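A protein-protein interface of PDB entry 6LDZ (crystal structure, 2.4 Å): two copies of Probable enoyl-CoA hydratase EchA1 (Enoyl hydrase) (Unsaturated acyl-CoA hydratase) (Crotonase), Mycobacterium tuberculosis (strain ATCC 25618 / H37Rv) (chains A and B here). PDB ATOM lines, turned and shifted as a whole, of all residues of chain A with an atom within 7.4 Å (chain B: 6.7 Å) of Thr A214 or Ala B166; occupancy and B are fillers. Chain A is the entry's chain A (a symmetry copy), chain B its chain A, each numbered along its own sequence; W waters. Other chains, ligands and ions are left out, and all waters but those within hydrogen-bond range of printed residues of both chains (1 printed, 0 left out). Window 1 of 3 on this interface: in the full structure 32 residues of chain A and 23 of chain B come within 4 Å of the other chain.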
ATOM      1  N   ILE A 203       6.912   2.480 -19.663  1.00  0.00           N
ATOM      2  CA  ILE A 203       8.361   2.445 -19.550  1.00  0.00           C
ATOM      3  C   ILE A 203       9.018   2.697 -20.908  1.00  0.00           C
ATOM      4  O   ILE A 203      10.003   3.443 -21.003  1.00  0.00           O
ATOM      5  CB  ILE A 203       8.807   1.121 -18.910  1.00  0.00           C
ATOM      6  CG1 ILE A 203       8.138   0.971 -17.535  1.00  0.00           C
ATOM      7  CG2 ILE A 203      10.322   1.083 -18.763  1.00  0.00           C
ATOM      8  CD1 ILE A 203       8.610  -0.207 -16.729  1.00  0.00           C
ATOM      9  N   ASN A 206       9.647   6.384 -22.079  1.00  0.00           N
ATOM     10  CA  ASN A 206      10.695   7.170 -21.444  1.00  0.00           C
ATOM     11  C   ASN A 206      12.039   6.921 -22.120  1.00  0.00           C
ATOM     12  O   ASN A 206      12.178   6.057 -22.987  1.00  0.00           O
ATOM     13  CB  ASN A 206      10.762   6.847 -19.950  1.00  0.00           C
ATOM     14  CG  ASN A 206       9.487   7.219 -19.245  1.00  0.00           C
ATOM     15  OD1 ASN A 206       8.839   8.175 -19.656  1.00  0.00           O
ATOM     16  ND2 ASN A 206       9.123   6.497 -18.179  1.00  0.00           N
ATOM     17  N   GLY A 207      13.034   7.709 -21.728  1.00  0.00           N
ATOM     18  CA  GLY A 207      14.334   7.658 -22.359  1.00  0.00           C
ATOM     19  C   GLY A 207      14.983   6.308 -22.174  1.00  0.00           C
ATOM     20  O   GLY A 207      15.250   5.885 -21.042  1.00  0.00           O
ATOM     21  N   PRO A 208      15.240   5.595 -23.290  1.00  0.00           N
ATOM     22  CA  PRO A 208      15.834   4.241 -23.192  1.00  0.00           C
ATOM     23  C   PRO A 208      17.114   4.182 -22.363  1.00  0.00           C
ATOM     24  O   PRO A 208      17.247   3.314 -21.492  1.00  0.00           O
ATOM     25  CB  PRO A 208      16.101   3.866 -24.661  1.00  0.00           C
ATOM     26  CG  PRO A 208      15.347   4.831 -25.487  1.00  0.00           C
ATOM     27  CD  PRO A 208      15.127   6.064 -24.686  1.00  0.00           C
ATOM     28  N   LEU A 209      18.069   5.084 -22.619  1.00  0.00           N
ATOM     29  CA  LEU A 209      19.298   5.120 -21.823  1.00  0.00           C
ATOM     30  C   LEU A 209      19.006   5.428 -20.356  1.00  0.00           C
ATOM     31  O   LEU A 209      19.623   4.844 -19.451  1.00  0.00           O
ATOM     32  CB  LEU A 209      20.277   6.162 -22.393  1.00  0.00           C
ATOM     33  CG  LEU A 209      20.761   6.021 -23.838  1.00  0.00           C
ATOM     34  CD1 LEU A 209      21.691   7.162 -24.165  1.00  0.00           C
ATOM     35  CD2 LEU A 209      21.445   4.679 -24.087  1.00  0.00           C
ATOM     36  N   ALA A 210      18.088   6.364 -20.100  1.00  0.00           N
ATOM     37  CA  ALA A 210      17.800   6.732 -18.719  1.00  0.00           C
ATOM     38  C   ALA A 210      17.079   5.604 -17.999  1.00  0.00           C
ATOM     39  O   ALA A 210      17.320   5.362 -16.810  1.00  0.00           O
ATOM     40  CB  ALA A 210      16.980   8.020 -18.670  1.00  0.00           C
ATOM     41  N   VAL A 211      16.214   4.883 -18.715  1.00  0.00           N
ATOM     42  CA  VAL A 211      15.538   3.730 -18.124  1.00  0.00           C
ATOM     43  C   VAL A 211      16.550   2.637 -17.779  1.00  0.00           C
ATOM     44  O   VAL A 211      16.560   2.107 -16.660  1.00  0.00           O
ATOM     45  CB  VAL A 211      14.435   3.214 -19.071  1.00  0.00           C
ATOM     46  CG1 VAL A 211      13.962   1.824 -18.653  1.00  0.00           C
ATOM     47  CG2 VAL A 211      13.255   4.202 -19.125  1.00  0.00           C
ATOM     48  N   VAL A 212      17.427   2.287 -18.732  1.00  0.00           N
ATOM     49  CA  VAL A 212      18.398   1.226 -18.465  1.00  0.00           C
ATOM     50  C   VAL A 212      19.380   1.662 -17.377  1.00  0.00           C
ATOM     51  O   VAL A 212      19.771   0.852 -16.525  1.00  0.00           O
ATOM     52  CB  VAL A 212      19.096   0.799 -19.773  1.00  0.00           C
ATOM     53  CG1 VAL A 212      20.369  -0.016 -19.502  1.00  0.00           C
ATOM     54  CG2 VAL A 212      18.134  -0.018 -20.635  1.00  0.00           C
ATOM     55  N   ALA A 213      19.730   2.956 -17.328  1.00  0.00           N
ATOM     56  CA  ALA A 213      20.636   3.438 -16.288  1.00  0.00           C
ATOM     57  C   ALA A 213      19.955   3.499 -14.919  1.00  0.00           C
ATOM     58  O   ALA A 213      20.606   3.288 -13.882  1.00  0.00           O
ATOM     59  CB  ALA A 213      21.186   4.809 -16.668  1.00  0.00           C
ATOM     60  N   THR A 214      18.655   3.797 -14.890  1.00  0.00           N
ATOM     61  CA  THR A 214      17.955   3.864 -13.613  1.00  0.00           C
ATOM     62  C   THR A 214      17.901   2.486 -12.978  1.00  0.00           C
ATOM     63  O   THR A 214      18.252   2.316 -11.804  1.00  0.00           O
ATOM     64  CB  THR A 214      16.553   4.457 -13.810  1.00  0.00           C
ATOM     65  OG1 THR A 214      16.680   5.817 -14.252  1.00  0.00           O
ATOM     66  CG2 THR A 214      15.749   4.444 -12.521  1.00  0.00           C
ATOM     67  N   LYS A 215      17.520   1.474 -13.756  1.00  0.00           N
ATOM     68  CA  LYS A 215      17.499   0.117 -13.216  1.00  0.00           C
ATOM     69  C   LYS A 215      18.899  -0.334 -12.790  1.00  0.00           C
ATOM     70  O   LYS A 215      19.074  -0.921 -11.715  1.00  0.00           O
ATOM     71  CB  LYS A 215      16.899  -0.848 -14.245  1.00  0.00           C
ATOM     72  CG  LYS A 215      17.354  -2.276 -14.059  1.00  0.00           C
ATOM     73  CD  LYS A 215      16.511  -3.271 -14.826  1.00  0.00           C
ATOM     74  CE  LYS A 215      16.996  -4.697 -14.524  1.00  0.00           C
ATOM     75  NZ  LYS A 215      16.674  -5.686 -15.614  1.00  0.00           N
ATOM     76  N   ARG A 216      19.910  -0.047 -13.609  1.00  0.00           N
ATOM     77  CA  ARG A 216      21.274  -0.432 -13.268  1.00  0.00           C
ATOM     78  C   ARG A 216      21.719   0.175 -11.934  1.00  0.00           C
ATOM     79  O   ARG A 216      22.381  -0.496 -11.134  1.00  0.00           O
ATOM     80  CB  ARG A 216      22.213  -0.026 -14.406  1.00  0.00           C
ATOM     81  CG  ARG A 216      23.666  -0.117 -14.060  1.00  0.00           C
ATOM     82  CD  ARG A 216      24.535   0.098 -15.274  1.00  0.00           C
ATOM     83  NE  ARG A 216      25.902  -0.281 -14.963  1.00  0.00           N
ATOM     84  CZ  ARG A 216      26.962   0.132 -15.642  1.00  0.00           C
ATOM     85  NH1 ARG A 216      26.809   0.947 -16.678  1.00  0.00           N
ATOM     86  NH2 ARG A 216      28.169  -0.279 -15.287  1.00  0.00           N
ATOM     87  N   ILE A 217      21.351   1.436 -11.666  1.00  0.00           N
ATOM     88  CA  ILE A 217      21.736   2.055 -10.399  1.00  0.00           C
ATOM     89  C   ILE A 217      21.017   1.382  -9.230  1.00  0.00           C
ATOM     90  O   ILE A 217      21.629   1.068  -8.205  1.00  0.00           O
ATOM     91  CB  ILE A 217      21.478   3.574 -10.432  1.00  0.00           C
ATOM     92  CG1 ILE A 217      22.528   4.268 -11.308  1.00  0.00           C
ATOM     93  CG2 ILE A 217      21.554   4.154  -9.028  1.00  0.00           C
ATOM     94  CD1 ILE A 217      22.165   5.705 -11.670  1.00  0.00           C
ATOM     95  N   ILE A 218      19.725   1.099  -9.381  1.00  0.00           N
ATOM     96  CA  ILE A 218      18.971   0.476  -8.296  1.00  0.00           C
ATOM     97  C   ILE A 218      19.477  -0.941  -8.012  1.00  0.00           C
ATOM     98  O   ILE A 218      19.670  -1.322  -6.850  1.00  0.00           O
ATOM     99  CB  ILE A 218      17.470   0.497  -8.622  1.00  0.00           C
ATOM    100  CG1 ILE A 218      16.938   1.923  -8.443  1.00  0.00           C
ATOM    101  CG2 ILE A 218      16.719  -0.491  -7.748  1.00  0.00           C
ATOM    102  CD1 ILE A 218      15.568   2.108  -8.961  1.00  0.00           C
ATOM    103  N   THR A 219      19.706  -1.742  -9.062  1.00  0.00           N
ATOM    104  CA  THR A 219      20.131  -3.129  -8.852  1.00  0.00           C
ATOM    105  C   THR A 219      21.561  -3.196  -8.325  1.00  0.00           C
ATOM    106  O   THR A 219      21.844  -3.939  -7.378  1.00  0.00           O
ATOM    107  CB  THR A 219      19.993  -3.960 -10.140  1.00  0.00           C
ATOM    108  OG1 THR A 219      20.845  -3.433 -11.165  1.00  0.00           O
ATOM    109  CG2 THR A 219      18.544  -3.982 -10.634  1.00  0.00           C
ATOM    110  N   GLU A 220      22.477  -2.420  -8.911  1.00  0.00           N
ATOM    111  CA  GLU A 220      23.870  -2.462  -8.475  1.00  0.00           C
ATOM    112  C   GLU A 220      24.118  -1.723  -7.161  1.00  0.00           C
ATOM    113  O   GLU A 220      25.144  -1.966  -6.513  1.00  0.00           O
ATOM    114  CB  GLU A 220      24.788  -1.893  -9.561  1.00  0.00           C
ATOM    115  CG  GLU A 220      24.772  -2.716 -10.847  1.00  0.00           C
ATOM    116  CD  GLU A 220      25.652  -2.136 -11.942  1.00  0.00           C
ATOM    117  OE1 GLU A 220      26.513  -1.280 -11.644  1.00  0.00           O
ATOM    118  OE2 GLU A 220      25.473  -2.541 -13.107  1.00  0.00           O
ATOM    119  N   ILE A 236      27.633   6.082 -13.746  1.00  0.00           N
ATOM    120  CA  ILE A 236      26.525   5.680 -14.609  1.00  0.00           C
ATOM    121  C   ILE A 236      25.771   6.900 -15.148  1.00  0.00           C
ATOM    122  O   ILE A 236      25.262   6.868 -16.276  1.00  0.00           O
ATOM    123  CB  ILE A 236      25.602   4.726 -13.827  1.00  0.00           C
ATOM    124  CG1 ILE A 236      26.363   3.445 -13.471  1.00  0.00           C
ATOM    125  CG2 ILE A 236      24.302   4.431 -14.595  1.00  0.00           C
ATOM    126  CD1 ILE A 236      25.797   2.701 -12.285  1.00  0.00           C
ATOM    127  N   LEU A 237      25.728   7.994 -14.368  1.00  0.00           N
ATOM    128  CA  LEU A 237      24.958   9.195 -14.694  1.00  0.00           C
ATOM    129  C   LEU A 237      25.559   9.984 -15.846  1.00  0.00           C
ATOM    130  O   LEU A 237      24.820  10.571 -16.651  1.00  0.00           O
ATOM    131  CB  LEU A 237      24.873  10.106 -13.469  1.00  0.00           C
ATOM    132  CG  LEU A 237      23.944   9.667 -12.351  1.00  0.00           C
ATOM    133  CD1 LEU A 237      23.571  10.824 -11.443  1.00  0.00           C
ATOM    134  CD2 LEU A 237      22.733   9.061 -12.977  1.00  0.00           C
ATOM    135  N   VAL A 240      24.490   9.220 -19.550  1.00  0.00           N
ATOM    136  CA  VAL A 240      23.102   9.595 -19.813  1.00  0.00           C
ATOM    137  C   VAL A 240      22.962  11.114 -19.930  1.00  0.00           C
ATOM    138  O   VAL A 240      22.258  11.618 -20.819  1.00  0.00           O
ATOM    139  CB  VAL A 240      22.187   9.018 -18.720  1.00  0.00           C
ATOM    140  CG1 VAL A 240      20.727   9.406 -18.960  1.00  0.00           C
ATOM    141  CG2 VAL A 240      22.340   7.501 -18.675  1.00  0.00           C
ATOM    142  N   ILE B 136       9.497  10.589  -9.012  1.00  0.00           N
ATOM    143  CA  ILE B 136      10.800  10.889  -9.623  1.00  0.00           C
ATOM    144  C   ILE B 136      10.690  10.772 -11.141  1.00  0.00           C
ATOM    145  O   ILE B 136      11.113   9.762 -11.726  1.00  0.00           O
ATOM    146  CB  ILE B 136      11.916   9.984  -9.075  1.00  0.00           C
ATOM    147  CG1 ILE B 136      11.457   8.522  -8.984  1.00  0.00           C
ATOM    148  CG2 ILE B 136      12.383  10.492  -7.699  1.00  0.00           C
ATOM    149  CD1 ILE B 136      12.592   7.564  -8.731  1.00  0.00           C
ATOM    150  N   PRO B 137      10.160  11.794 -11.823  1.00  0.00           N
ATOM    151  CA  PRO B 137       9.892  11.666 -13.265  1.00  0.00           C
ATOM    152  C   PRO B 137      11.090  11.915 -14.186  1.00  0.00           C
ATOM    153  O   PRO B 137      10.902  12.122 -15.387  1.00  0.00           O
ATOM    154  CB  PRO B 137       8.790  12.709 -13.494  1.00  0.00           C
ATOM    155  CG  PRO B 137       9.092  13.791 -12.463  1.00  0.00           C
ATOM    156  CD  PRO B 137       9.735  13.101 -11.278  1.00  0.00           C
ATOM    157  N   GLU B 138      12.318  11.840 -13.667  1.00  0.00           N
ATOM    158  CA  GLU B 138      13.490  12.212 -14.465  1.00  0.00           C
ATOM    159  C   GLU B 138      13.565  11.450 -15.792  1.00  0.00           C
ATOM    160  O   GLU B 138      13.907  12.035 -16.828  1.00  0.00           O
ATOM    161  CB  GLU B 138      14.774  11.987 -13.656  1.00  0.00           C
ATOM    162  CG  GLU B 138      15.138  13.147 -12.700  1.00  0.00           C
ATOM    163  CD  GLU B 138      14.415  13.069 -11.348  1.00  0.00           C
ATOM    164  OE1 GLU B 138      13.376  12.379 -11.253  1.00  0.00           O
ATOM    165  OE2 GLU B 138      14.898  13.691 -10.369  1.00  0.00           O
ATOM    166  N   VAL B 139      13.251  10.144 -15.786  1.00  0.00           N
ATOM    167  CA  VAL B 139      13.406   9.354 -17.008  1.00  0.00           C
ATOM    168  C   VAL B 139      12.506   9.868 -18.127  1.00  0.00           C
ATOM    169  O   VAL B 139      12.835   9.715 -19.312  1.00  0.00           O
ATOM    170  CB  VAL B 139      13.142   7.847 -16.745  1.00  0.00           C
ATOM    171  CG1 VAL B 139      14.237   7.243 -15.846  1.00  0.00           C
ATOM    172  CG2 VAL B 139      11.714   7.612 -16.155  1.00  0.00           C
ATOM    173  N   LYS B 140      11.378  10.498 -17.779  1.00  0.00           N
ATOM    174  CA  LYS B 140      10.501  11.078 -18.786  1.00  0.00           C
ATOM    175  C   LYS B 140      11.204  12.149 -19.614  1.00  0.00           C
ATOM    176  O   LYS B 140      10.779  12.415 -20.740  1.00  0.00           O
ATOM    177  CB  LYS B 140       9.261  11.682 -18.120  1.00  0.00           C
ATOM    178  CG  LYS B 140       8.270  10.672 -17.553  1.00  0.00           C
ATOM    179  CD  LYS B 140       7.391  11.372 -16.546  1.00  0.00           C
ATOM    180  CE  LYS B 140       5.929  11.149 -16.819  1.00  0.00           C
ATOM    181  NZ  LYS B 140       5.333  10.129 -15.904  1.00  0.00           N
ATOM    182  N   LEU B 143      16.585  11.697 -18.376  1.00  0.00           N
ATOM    183  CA  LEU B 143      17.541  11.936 -17.307  1.00  0.00           C
ATOM    184  C   LEU B 143      17.365  10.872 -16.223  1.00  0.00           C
ATOM    185  O   LEU B 143      16.507   9.993 -16.314  1.00  0.00           O
ATOM    186  CB  LEU B 143      17.377  13.356 -16.743  1.00  0.00           C
ATOM    187  CG  LEU B 143      17.705  14.484 -17.738  1.00  0.00           C
ATOM    188  CD1 LEU B 143      17.508  15.883 -17.128  1.00  0.00           C
ATOM    189  CD2 LEU B 143      19.123  14.330 -18.300  1.00  0.00           C
ATOM    190  N   VAL B 144      18.197  10.954 -15.192  1.00  0.00           N
ATOM    191  CA  VAL B 144      18.177  10.018 -14.075  1.00  0.00           C
ATOM    192  C   VAL B 144      18.147  10.826 -12.785  1.00  0.00           C
ATOM    193  O   VAL B 144      18.760  11.895 -12.706  1.00  0.00           O
ATOM    194  CB  VAL B 144      19.406   9.073 -14.112  1.00  0.00           C
ATOM    195  CG1 VAL B 144      19.480   8.213 -12.872  1.00  0.00           C
ATOM    196  CG2 VAL B 144      19.364   8.191 -15.346  1.00  0.00           C
ATOM    197  N   ALA B 145      17.427  10.327 -11.777  1.00  0.00           N
ATOM    198  CA  ALA B 145      17.398  10.992 -10.476  1.00  0.00           C
ATOM    199  C   ALA B 145      18.696  10.706  -9.712  1.00  0.00           C
ATOM    200  O   ALA B 145      18.908   9.592  -9.210  1.00  0.00           O
ATOM    201  CB  ALA B 145      16.181  10.536  -9.683  1.00  0.00           C
ATOM    202  N   LEU B 150      17.331   7.126  -6.152  1.00  0.00           N
ATOM    203  CA  LEU B 150      17.533   5.739  -6.543  1.00  0.00           C
ATOM    204  C   LEU B 150      18.244   4.924  -5.475  1.00  0.00           C
ATOM    205  O   LEU B 150      18.191   3.693  -5.526  1.00  0.00           O
ATOM    206  CB  LEU B 150      18.321   5.670  -7.850  1.00  0.00           C
ATOM    207  CG  LEU B 150      17.644   6.414  -8.997  1.00  0.00           C
ATOM    208  CD1 LEU B 150      18.395   6.177 -10.302  1.00  0.00           C
ATOM    209  CD2 LEU B 150      16.167   6.018  -9.113  1.00  0.00           C
ATOM    210  N   LEU B 153      14.912   5.367  -2.002  1.00  0.00           N
ATOM    211  CA  LEU B 153      13.545   4.880  -2.191  1.00  0.00           C
ATOM    212  C   LEU B 153      13.440   3.364  -2.058  1.00  0.00           C
ATOM    213  O   LEU B 153      12.552   2.898  -1.323  1.00  0.00           O
ATOM    214  CB  LEU B 153      13.005   5.375  -3.543  1.00  0.00           C
ATOM    215  CG  LEU B 153      11.493   5.314  -3.813  1.00  0.00           C
ATOM    216  CD1 LEU B 153      10.667   5.984  -2.702  1.00  0.00           C
ATOM    217  CD2 LEU B 153      11.138   5.892  -5.196  1.00  0.00           C
ATOM    218  N   ILE B 161       8.030  -1.458  -5.927  1.00  0.00           N
ATOM    219  CA  ILE B 161       7.328  -0.182  -6.093  1.00  0.00           C
ATOM    220  C   ILE B 161       8.321   0.947  -6.393  1.00  0.00           C
ATOM    221  O   ILE B 161       8.090   1.780  -7.280  1.00  0.00           O
ATOM    222  CB  ILE B 161       6.467   0.141  -4.853  1.00  0.00           C
ATOM    223  CG1 ILE B 161       5.673  -1.090  -4.377  1.00  0.00           C
ATOM    224  CG2 ILE B 161       5.533   1.321  -5.164  1.00  0.00           C
ATOM    225  CD1 ILE B 161       4.873  -1.768  -5.475  1.00  0.00           C
ATOM    226  N   ALA B 162       9.421   1.013  -5.633  1.00  0.00           N
ATOM    227  CA  ALA B 162      10.472   1.977  -5.933  1.00  0.00           C
ATOM    228  C   ALA B 162      10.935   1.827  -7.376  1.00  0.00           C
ATOM    229  O   ALA B 162      11.107   2.823  -8.097  1.00  0.00           O
ATOM    230  CB  ALA B 162      11.650   1.787  -4.970  1.00  0.00           C
ATOM    231  N   MET B 163      11.108   0.578  -7.826  1.00  0.00           N
ATOM    232  CA  MET B 163      11.560   0.351  -9.193  1.00  0.00           C
ATOM    233  C   MET B 163      10.531   0.859 -10.190  1.00  0.00           C
ATOM    234  O   MET B 163      10.885   1.531 -11.172  1.00  0.00           O
ATOM    235  CB  MET B 163      11.850  -1.138  -9.412  1.00  0.00           C
ATOM    236  CG  MET B 163      12.128  -1.481 -10.833  1.00  0.00           C
ATOM    237  SD  MET B 163      13.849  -1.125 -11.282  1.00  0.00           S
ATOM    238  CE  MET B 163      14.733  -2.379 -10.296  1.00  0.00           C
ATOM    239  N   GLU B 164       9.244   0.590  -9.923  1.00  0.00           N
ATOM    240  CA  GLU B 164       8.176   1.048 -10.816  1.00  0.00           C
ATOM    241  C   GLU B 164       8.155   2.578 -10.955  1.00  0.00           C
ATOM    242  O   GLU B 164       8.097   3.125 -12.074  1.00  0.00           O
ATOM    243  CB  GLU B 164       6.837   0.540 -10.295  1.00  0.00           C
ATOM    244  CG  GLU B 164       5.634   1.047 -11.069  1.00  0.00           C
ATOM    245  CD  GLU B 164       4.303   0.756 -10.388  1.00  0.00           C
ATOM    246  OE1 GLU B 164       4.257   0.225  -9.255  1.00  0.00           O
ATOM    247  OE2 GLU B 164       3.284   1.073 -11.022  1.00  0.00           O
ATOM    248  N   LEU B 165       8.176   3.286  -9.821  1.00  0.00           N
ATOM    249  CA  LEU B 165       8.160   4.741  -9.854  1.00  0.00           C
ATOM    250  C   LEU B 165       9.376   5.277 -10.596  1.00  0.00           C
ATOM    251  O   LEU B 165       9.271   6.251 -11.354  1.00  0.00           O
ATOM    252  CB  LEU B 165       8.106   5.283  -8.425  1.00  0.00           C
ATOM    253  CG  LEU B 165       6.802   5.031  -7.685  1.00  0.00           C
ATOM    254  CD1 LEU B 165       6.999   5.286  -6.213  1.00  0.00           C
ATOM    255  CD2 LEU B 165       5.694   5.903  -8.248  1.00  0.00           C
ATOM    256  N   ALA B 166      10.526   4.627 -10.424  1.00  0.00           N
ATOM    257  CA  ALA B 166      11.745   5.083 -11.091  1.00  0.00           C
ATOM    258  C   ALA B 166      11.668   4.876 -12.603  1.00  0.00           C
ATOM    259  O   ALA B 166      12.125   5.728 -13.381  1.00  0.00           O
ATOM    260  CB  ALA B 166      12.956   4.355 -10.497  1.00  0.00           C
ATOM    261  N   LEU B 167      11.080   3.756 -13.037  1.00  0.00           N
ATOM    262  CA  LEU B 167      11.052   3.422 -14.461  1.00  0.00           C
ATOM    263  C   LEU B 167       9.943   4.163 -15.190  1.00  0.00           C
ATOM    264  O   LEU B 167      10.118   4.536 -16.355  1.00  0.00           O
ATOM    265  CB  LEU B 167      10.905   1.906 -14.645  1.00  0.00           C
ATOM    266  CG  LEU B 167      12.135   1.109 -14.186  1.00  0.00           C
ATOM    267  CD1 LEU B 167      12.079  -0.351 -14.646  1.00  0.00           C
ATOM    268  CD2 LEU B 167      13.426   1.783 -14.670  1.00  0.00           C
ATOM    269  N   THR B 168       8.803   4.398 -14.528  1.00  0.00           N
ATOM    270  CA  THR B 168       7.701   5.090 -15.192  1.00  0.00           C
ATOM    271  C   THR B 168       7.746   6.598 -15.007  1.00  0.00           C
ATOM    272  O   THR B 168       7.258   7.328 -15.876  1.00  0.00           O
ATOM    273  CB  THR B 168       6.332   4.603 -14.689  1.00  0.00           C
ATOM    274  OG1 THR B 168       6.170   4.986 -13.311  1.00  0.00           O
ATOM    275  CG2 THR B 168       6.161   3.103 -14.847  1.00  0.00           C
ATOM    276  N   GLY B 169       8.307   7.092 -13.903  1.00  0.00           N
ATOM    277  CA  GLY B 169       8.133   8.505 -13.596  1.00  0.00           C
ATOM    278  C   GLY B 169       6.781   8.866 -13.015  1.00  0.00           C
ATOM    279  O   GLY B 169       6.513  10.053 -12.818  1.00  0.00           O
ATOM    280  N   ASP B 170       5.922   7.883 -12.731  1.00  0.00           N
ATOM    281  CA  ASP B 170       4.572   8.142 -12.245  1.00  0.00           C
ATOM    282  C   ASP B 170       4.592   8.832 -10.886  1.00  0.00           C
ATOM    283  O   ASP B 170       5.561   8.752 -10.132  1.00  0.00           O
ATOM    284  CB  ASP B 170       3.782   6.842 -12.104  1.00  0.00           C
ATOM    285  CG  ASP B 170       3.187   6.372 -13.412  1.00  0.00           C
ATOM    286  OD1 ASP B 170       3.245   7.140 -14.400  1.00  0.00           O
ATOM    287  OD2 ASP B 170       2.648   5.241 -13.435  1.00  0.00           O
HETATM  288  O   HOH W   1      15.849   7.966 -12.613  1.00  0.00           O
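ND2 of Asn A206 is in hydrogen-bond range of O of Leu B167 (2.9 Å).
The backbone carbonyl oxygen (O) of Thr B168 lies within hydrogen-bond range of the side-chain amide nitrogen (ND2) of Asn A206, at 3.1 Å.
O of Val B139 is in hydrogen-bond range of N of Gly A207 (3.1 Å).
The side-chain hydroxyl (OG1) of Thr B168 sits at hydrogen-bond distance from the backbone carbonyl oxygen (O) of Glu B164 (3.0 Å).
O of Ala A210 is in hydrogen-bond range of OG1 of Thr A214 (2.7 Å).
N of Asp B170 lies within hydrogen-bond range of OG1 of Thr B168, 3.0 Å away.
The backbone carbonyl oxygen of Thr B168 sits at hydrogen-bond distance from the side-chain amino group of Lys B140, at 3.4 Å.
The backbone carbonyl oxygen (O) of Glu B138 sits at hydrogen-bond distance from the backbone NH (N) of Leu B143 (3.1 Å).
NZ of Lys B140 lies within salt-bridge range of OD1 of Asp B170.
Among the printed residues, merely in contact across the chains: Ile A203 with Leu B167, Ile A203 with Thr B168, Asn A206 with Val B139, Asn A206 with Lys B140, Ala A210 with Val B139, Ala A210 with Leu B143, Ala A210 with Val B144, Val A211 with Leu B167, Thr A214 with Val B139, Thr A214 with Val B144, Thr A214 with Leu B150, Thr A214 with Ala B166, Ile A217 with Val B144, Ile A217 with Leu B150, Ile A218 with Leu B150, Ile A218 with Met B163, Ile A218 with Ala B166 and Leu A237 with Val B144.
Printed residues of chain B within 4 Å of Gly A207: Val B139.
Of chain B, only Val B139, Val B144, Leu B150 and Ala B166 come within 4 Å of Thr A214.
Of the printed residues of chain B, Ile A218 touches Leu B150, Met B163 and Ala B166.
Of chain A, only Thr A214 and Ile A218 come within 4 Å of Ala B166.
The nearest residue of chain B that does not touch Thr A214 is Leu B167 (4.1 Å).
The nearest printed residue of chain B that does not touch Ile A217 is Ala B145 (5.6 Å).
Of the 19 printed residues of chain A, 9 touch a printed residue of chain B.
Printed residues of chain A that touch a printed residue of chain B: Ile A203, Asn A206, Gly A207, Ala A210, Val A211, Thr A214, Ile A217, Ile A218 and Leu A237.
Printed residues of chain B that touch a printed residue of chain A: Val B139, Lys B140, Leu B143, Val B144, Leu B150, Met B163, Ala B166, Leu B167 and Thr B168.
Hydrophobic or aromatic side chains of chain B within 4 Å of the printed part of chain A: Val B139, Val B144, Leu B150, Met B163, Ala B166 and Leu B167.
Among the printed residues, no Asp or Glu carboxylate lies within 4 Å of a Lys or Arg side-chain nitrogen of the other chain.
No position is printed for both chains.
Water W1 bridges the side-chain hydroxyl of Thr A214 (2.8 Å) and the backbone NH of Ala B145 (3.0 Å).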
